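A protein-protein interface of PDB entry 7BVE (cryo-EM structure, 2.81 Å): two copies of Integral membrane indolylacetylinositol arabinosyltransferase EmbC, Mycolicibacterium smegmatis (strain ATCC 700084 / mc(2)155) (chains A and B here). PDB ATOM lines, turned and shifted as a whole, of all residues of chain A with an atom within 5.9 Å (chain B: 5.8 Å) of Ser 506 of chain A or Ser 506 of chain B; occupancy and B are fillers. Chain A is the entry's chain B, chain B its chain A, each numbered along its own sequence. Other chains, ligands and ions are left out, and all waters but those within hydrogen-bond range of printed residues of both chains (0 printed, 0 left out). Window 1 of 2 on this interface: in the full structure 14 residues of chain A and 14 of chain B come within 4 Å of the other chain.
His 502 of chain A touches Phe 509 of chain B, and with the chains exchanged Phe 509 of chain A touches His 502 of chain B.
Ser 506 of chain B touches its own counterpart, Ser 506 of chain A.
9 positions are printed for both chains.
Of the 3 pairs that touch across the chains among the printed residues, 3 have their exchanged pair printed and touching as well.
Of the 9 printed residues of chain A, 3 touch a printed residue of chain B.
Hydrophobic or aromatic side chains of chain B that line the printed part of chain A: His 502 and Phe 509.
Among the printed residues, no Asp or Glu carboxylate lies within 4 Å of a Lys or Arg side-chain nitrogen of the other chain.
The side-chain hydroxyl (OG) of Ser 506 of chain A lies within hydrogen-bond range of the backbone carbonyl oxygen (O) of His 502 of chain A (2.9 Å).
The backbone carbonyl oxygen (O) of His 502 of chain B lies within hydrogen-bond range of the side-chain hydroxyl (OG) of Ser 506 of chain B.
Printed residues of chain B within 4 Å of His 502 of chain A: Phe 509.
Leu 508 of chain A touches none of the printed residues of chain B.
Of the printed residues of chain B, Phe 509 of chain A touches His 502 (3.1 Å).
Printed residues of chain A within 4 Å of His 502 of chain B: Phe 509 (3.1 Å).
Ser 506 of chain B touches just one residue of chain A: Ser 506 (3.7 Å).
Printed residues of chain A within 4 Å of Phe 509 of chain B: His 502.
The nearest printed residue of chain B that does not touch His 502 of chain A is Thr 510 of chain B (5.3 Å).
A ring nitrogen (NE2) of His 502 of chain A is in hydrogen-bond range of the backbone carbonyl oxygen (O) of Phe 509 of chain B (3.2 Å).
The backbone carbonyl oxygen of Phe 509 of chain A is in hydrogen-bond range of a ring nitrogen (NE2) of His 502 of chain B, 3.1 Å away.
Among the printed residues, merely in contact across the chains: Ser 506 of chain A with Ser 506 of chain B.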
ATOM      1  N   HIS A 502      18.606   5.170  -8.128  1.00  0.00           N
ATOM      2  CA  HIS A 502      18.463   6.487  -8.737  1.00  0.00           C
ATOM      3  C   HIS A 502      17.587   7.428  -7.919  1.00  0.00           C
ATOM      4  O   HIS A 502      17.630   8.639  -8.146  1.00  0.00           O
ATOM      5  CB  HIS A 502      17.886   6.357 -10.144  1.00  0.00           C
ATOM      6  CG  HIS A 502      16.488   5.827 -10.180  1.00  0.00           C
ATOM      7  ND1 HIS A 502      16.200   4.481 -10.180  1.00  0.00           N
ATOM      8  CD2 HIS A 502      15.297   6.466 -10.205  1.00  0.00           C
ATOM      9  CE1 HIS A 502      14.892   4.313 -10.210  1.00  0.00           C
ATOM     10  NE2 HIS A 502      14.321   5.502 -10.223  1.00  0.00           N
ATOM     11  N   ILE A 503      16.804   6.903  -6.975  1.00  0.00           N
ATOM     12  CA  ILE A 503      15.890   7.718  -6.181  1.00  0.00           C
ATOM     13  C   ILE A 503      16.651   8.612  -5.213  1.00  0.00           C
ATOM     14  O   ILE A 503      16.225   9.740  -4.940  1.00  0.00           O
ATOM     15  CB  ILE A 503      14.881   6.787  -5.485  1.00  0.00           C
ATOM     16  CG1 ILE A 503      13.999   6.134  -6.539  1.00  0.00           C
ATOM     17  CG2 ILE A 503      14.001   7.507  -4.493  1.00  0.00           C
ATOM     18  CD1 ILE A 503      13.098   5.071  -6.013  1.00  0.00           C
ATOM     19  N   ARG A 504      17.814   8.166  -4.736  1.00  0.00           N
ATOM     20  CA  ARG A 504      18.641   8.999  -3.867  1.00  0.00           C
ATOM     21  C   ARG A 504      19.148  10.242  -4.595  1.00  0.00           C
ATOM     22  O   ARG A 504      19.110  11.352  -4.055  1.00  0.00           O
ATOM     23  CB  ARG A 504      19.799   8.170  -3.320  1.00  0.00           C
ATOM     24  CG  ARG A 504      20.735   8.936  -2.432  1.00  0.00           C
ATOM     25  CD  ARG A 504      21.835   8.084  -1.845  1.00  0.00           C
ATOM     26  NE  ARG A 504      21.401   7.199  -0.770  1.00  0.00           N
ATOM     27  CZ  ARG A 504      21.465   5.880  -0.808  1.00  0.00           C
ATOM     28  NH1 ARG A 504      21.944   5.267  -1.876  1.00  0.00           N
ATOM     29  NH2 ARG A 504      21.051   5.170   0.223  1.00  0.00           N
ATOM     30  N   TYR A 505      19.533  10.092  -5.855  1.00  0.00           N
ATOM     31  CA  TYR A 505      20.007  11.228  -6.633  1.00  0.00           C
ATOM     32  C   TYR A 505      18.860  12.083  -7.150  1.00  0.00           C
ATOM     33  O   TYR A 505      19.007  13.307  -7.270  1.00  0.00           O
ATOM     34  CB  TYR A 505      20.882  10.716  -7.770  1.00  0.00           C
ATOM     35  CG  TYR A 505      22.116  10.036  -7.241  1.00  0.00           C
ATOM     36  CD1 TYR A 505      23.232  10.772  -6.881  1.00  0.00           C
ATOM     37  CD2 TYR A 505      22.147   8.661  -7.050  1.00  0.00           C
ATOM     38  CE1 TYR A 505      24.349  10.158  -6.376  1.00  0.00           C
ATOM     39  CE2 TYR A 505      23.253   8.043  -6.539  1.00  0.00           C
ATOM     40  CZ  TYR A 505      24.351   8.793  -6.206  1.00  0.00           C
ATOM     41  OH  TYR A 505      25.462   8.168  -5.701  1.00  0.00           O
ATOM     42  N   SER A 506      17.711  11.465  -7.428  1.00  0.00           N
ATOM     43  CA  SER A 506      16.515  12.223  -7.773  1.00  0.00           C
ATOM     44  C   SER A 506      16.051  13.090  -6.614  1.00  0.00           C
ATOM     45  O   SER A 506      15.518  14.181  -6.829  1.00  0.00           O
ATOM     46  CB  SER A 506      15.402  11.271  -8.198  1.00  0.00           C
ATOM     47  OG  SER A 506      15.763  10.559  -9.365  1.00  0.00           O
ATOM     48  N   ARG A 507      16.234  12.623  -5.378  1.00  0.00           N
ATOM     49  CA  ARG A 507      15.951  13.458  -4.217  1.00  0.00           C
ATOM     50  C   ARG A 507      17.031  14.499  -3.991  1.00  0.00           C
ATOM     51  O   ARG A 507      16.741  15.568  -3.453  1.00  0.00           O
ATOM     52  CB  ARG A 507      15.799  12.607  -2.960  1.00  0.00           C
ATOM     53  CG  ARG A 507      14.564  11.757  -2.948  1.00  0.00           C
ATOM     54  CD  ARG A 507      14.465  10.904  -1.702  1.00  0.00           C
ATOM     55  NE  ARG A 507      13.337   9.983  -1.801  1.00  0.00           N
ATOM     56  CZ  ARG A 507      13.045   9.051  -0.904  1.00  0.00           C
ATOM     57  NH1 ARG A 507      13.793   8.910   0.176  1.00  0.00           N
ATOM     58  NH2 ARG A 507      12.001   8.258  -1.087  1.00  0.00           N
ATOM     59  N   LEU A 508      18.274  14.196  -4.361  1.00  0.00           N
ATOM     60  CA  LEU A 508      19.336  15.192  -4.282  1.00  0.00           C
ATOM     61  C   LEU A 508      19.105  16.359  -5.228  1.00  0.00           C
ATOM     62  O   LEU A 508      19.525  17.478  -4.925  1.00  0.00           O
ATOM     63  CB  LEU A 508      20.685  14.542  -4.580  1.00  0.00           C
ATOM     64  CG  LEU A 508      21.967  15.368  -4.470  1.00  0.00           C
ATOM     65  CD1 LEU A 508      22.206  15.793  -3.053  1.00  0.00           C
ATOM     66  CD2 LEU A 508      23.144  14.596  -4.993  1.00  0.00           C
ATOM     67  N   PHE A 509      18.439  16.136  -6.358  1.00  0.00           N
ATOM     68  CA  PHE A 509      18.167  17.213  -7.304  1.00  0.00           C
ATOM     69  C   PHE A 509      16.740  17.743  -7.230  1.00  0.00           C
ATOM     70  O   PHE A 509      16.180  18.148  -8.243  1.00  0.00           O
ATOM     71  CB  PHE A 509      18.483  16.769  -8.726  1.00  0.00           C
ATOM     72  CG  PHE A 509      19.938  16.671  -9.005  1.00  0.00           C
ATOM     73  CD1 PHE A 509      20.672  17.808  -9.270  1.00  0.00           C
ATOM     74  CD2 PHE A 509      20.576  15.453  -9.006  1.00  0.00           C
ATOM     75  CE1 PHE A 509      22.010  17.731  -9.521  1.00  0.00           C
ATOM     76  CE2 PHE A 509      21.915  15.367  -9.255  1.00  0.00           C
ATOM     77  CZ  PHE A 509      22.634  16.507  -9.514  1.00  0.00           C
ATOM     78  N   THR A 510      16.142  17.771  -6.048  1.00  0.00           N
ATOM     79  CA  THR A 510      14.856  18.430  -5.869  1.00  0.00           C
ATOM     80  C   THR A 510      15.072  19.875  -5.434  1.00  0.00           C
ATOM     81  O   THR A 510      16.181  20.406  -5.489  1.00  0.00           O
ATOM     82  CB  THR A 510      13.986  17.684  -4.863  1.00  0.00           C
ATOM     83  OG1 THR A 510      14.715  17.477  -3.649  1.00  0.00           O
ATOM     84  CG2 THR A 510      13.516  16.368  -5.421  1.00  0.00           C
ATOM     85  N   HIS B 502      18.583  16.867 -15.197  1.00  0.00           N
ATOM     86  CA  HIS B 502      18.376  15.609 -14.492  1.00  0.00           C
ATOM     87  C   HIS B 502      16.997  15.009 -14.734  1.00  0.00           C
ATOM     88  O   HIS B 502      16.793  13.836 -14.427  1.00  0.00           O
ATOM     89  CB  HIS B 502      18.583  15.801 -12.992  1.00  0.00           C
ATOM     90  CG  HIS B 502      17.563  16.685 -12.347  1.00  0.00           C
ATOM     91  ND1 HIS B 502      17.679  18.056 -12.312  1.00  0.00           N
ATOM     92  CD2 HIS B 502      16.402  16.391 -11.721  1.00  0.00           C
ATOM     93  CE1 HIS B 502      16.636  18.568 -11.686  1.00  0.00           C
ATOM     94  NE2 HIS B 502      15.844  17.579 -11.321  1.00  0.00           N
ATOM     95  N   ILE B 503      16.051  15.779 -15.276  1.00  0.00           N
ATOM     96  CA  ILE B 503      14.690  15.294 -15.483  1.00  0.00           C
ATOM     97  C   ILE B 503      14.633  14.283 -16.620  1.00  0.00           C
ATOM     98  O   ILE B 503      13.853  13.326 -16.566  1.00  0.00           O
ATOM     99  CB  ILE B 503      13.761  16.504 -15.698  1.00  0.00           C
ATOM    100  CG1 ILE B 503      13.683  17.303 -14.405  1.00  0.00           C
ATOM    101  CG2 ILE B 503      12.366  16.108 -16.115  1.00  0.00           C
ATOM    102  CD1 ILE B 503      12.958  18.599 -14.526  1.00  0.00           C
ATOM    103  N   ARG B 504      15.489  14.437 -17.632  1.00  0.00           N
ATOM    104  CA  ARG B 504      15.577  13.448 -18.704  1.00  0.00           C
ATOM    105  C   ARG B 504      16.044  12.093 -18.179  1.00  0.00           C
ATOM    106  O   ARG B 504      15.490  11.046 -18.541  1.00  0.00           O
ATOM    107  CB  ARG B 504      16.510  13.967 -19.794  1.00  0.00           C
ATOM    108  CG  ARG B 504      16.703  13.022 -20.943  1.00  0.00           C
ATOM    109  CD  ARG B 504      17.592  13.582 -22.033  1.00  0.00           C
ATOM    110  NE  ARG B 504      16.958  14.603 -22.857  1.00  0.00           N
ATOM    111  CZ  ARG B 504      17.377  15.853 -22.961  1.00  0.00           C
ATOM    112  NH1 ARG B 504      18.442  16.256 -22.291  1.00  0.00           N
ATOM    113  NH2 ARG B 504      16.735  16.703 -23.739  1.00  0.00           N
ATOM    114  N   TYR B 505      17.006  12.100 -17.266  1.00  0.00           N
ATOM    115  CA  TYR B 505      17.505  10.863 -16.684  1.00  0.00           C
ATOM    116  C   TYR B 505      16.605  10.349 -15.574  1.00  0.00           C
ATOM    117  O   TYR B 505      16.672   9.171 -15.229  1.00  0.00           O
ATOM    118  CB  TYR B 505      18.921  11.083 -16.173  1.00  0.00           C
ATOM    119  CG  TYR B 505      19.871  11.390 -17.295  1.00  0.00           C
ATOM    120  CD1 TYR B 505      20.436  10.372 -18.046  1.00  0.00           C
ATOM    121  CD2 TYR B 505      20.168  12.699 -17.635  1.00  0.00           C
ATOM    122  CE1 TYR B 505      21.288  10.651 -19.082  1.00  0.00           C
ATOM    123  CE2 TYR B 505      21.010  12.984 -18.667  1.00  0.00           C
ATOM    124  CZ  TYR B 505      21.568  11.962 -19.388  1.00  0.00           C
ATOM    125  OH  TYR B 505      22.418  12.264 -20.422  1.00  0.00           O
ATOM    126  N   SER B 506      15.768  11.207 -14.999  1.00  0.00           N
ATOM    127  CA  SER B 506      14.753  10.729 -14.075  1.00  0.00           C
ATOM    128  C   SER B 506      13.625  10.038 -14.823  1.00  0.00           C
ATOM    129  O   SER B 506      13.029   9.086 -14.315  1.00  0.00           O
ATOM    130  CB  SER B 506      14.213  11.888 -13.244  1.00  0.00           C
ATOM    131  OG  SER B 506      15.235  12.451 -12.442  1.00  0.00           O
ATOM    132  N   ARG B 507      13.311  10.511 -16.030  1.00  0.00           N
ATOM    133  CA  ARG B 507      12.304   9.854 -16.855  1.00  0.00           C
ATOM    134  C   ARG B 507      12.827   8.578 -17.485  1.00  0.00           C
ATOM    135  O   ARG B 507      12.034   7.688 -17.798  1.00  0.00           O
ATOM    136  CB  ARG B 507      11.808  10.791 -17.952  1.00  0.00           C
ATOM    137  CG  ARG B 507      11.003  11.949 -17.443  1.00  0.00           C
ATOM    138  CD  ARG B 507      10.548  12.867 -18.557  1.00  0.00           C
ATOM    139  NE  ARG B 507       9.907  14.057 -18.008  1.00  0.00           N
ATOM    140  CZ  ARG B 507       9.476  15.083 -18.732  1.00  0.00           C
ATOM    141  NH1 ARG B 507       9.606  15.067 -20.047  1.00  0.00           N
ATOM    142  NH2 ARG B 507       8.913  16.123 -18.140  1.00  0.00           N
ATOM    143  N   LEU B 508      14.139   8.474 -17.700  1.00  0.00           N
ATOM    144  CA  LEU B 508      14.701   7.230 -18.215  1.00  0.00           C
ATOM    145  C   LEU B 508      14.584   6.080 -17.221  1.00  0.00           C
ATOM    146  O   LEU B 508      14.542   4.920 -17.635  1.00  0.00           O
ATOM    147  CB  LEU B 508      16.164   7.446 -18.598  1.00  0.00           C
ATOM    148  CG  LEU B 508      16.963   6.336 -19.277  1.00  0.00           C
ATOM    149  CD1 LEU B 508      16.388   6.026 -20.625  1.00  0.00           C
ATOM    150  CD2 LEU B 508      18.409   6.723 -19.400  1.00  0.00           C
ATOM    151  N   PHE B 509      14.505   6.368 -15.923  1.00  0.00           N
ATOM    152  CA  PHE B 509      14.434   5.343 -14.891  1.00  0.00           C
ATOM    153  C   PHE B 509      13.055   5.234 -14.256  1.00  0.00           C
ATOM    154  O   PHE B 509      12.940   4.870 -13.089  1.00  0.00           O
ATOM    155  CB  PHE B 509      15.479   5.594 -13.812  1.00  0.00           C
ATOM    156  CG  PHE B 509      16.863   5.262 -14.237  1.00  0.00           C
ATOM    157  CD1 PHE B 509      17.300   3.952 -14.225  1.00  0.00           C
ATOM    158  CD2 PHE B 509      17.732   6.247 -14.644  1.00  0.00           C
ATOM    159  CE1 PHE B 509      18.567   3.637 -14.619  1.00  0.00           C
ATOM    160  CE2 PHE B 509      19.002   5.938 -15.041  1.00  0.00           C
ATOM    161  CZ  PHE B 509      19.420   4.630 -15.028  1.00  0.00           C
ATOM    162  N   THR B 510      12.004   5.526 -15.000  1.00  0.00           N
ATOM    163  CA  THR B 510      10.656   5.279 -14.521  1.00  0.00           C
ATOM    164  C   THR B 510      10.224   3.878 -14.938  1.00  0.00           C
ATOM    165  O   THR B 510      11.026   3.074 -15.414  1.00  0.00           O
ATOM    166  CB  THR B 510       9.692   6.341 -15.037  1.00  0.00           C
ATOM    167  OG1 THR B 510       9.765   6.404 -16.465  1.00  0.00           O
ATOM    168  CG2 THR B 510      10.017   7.689 -14.448  1.00  0.00           C
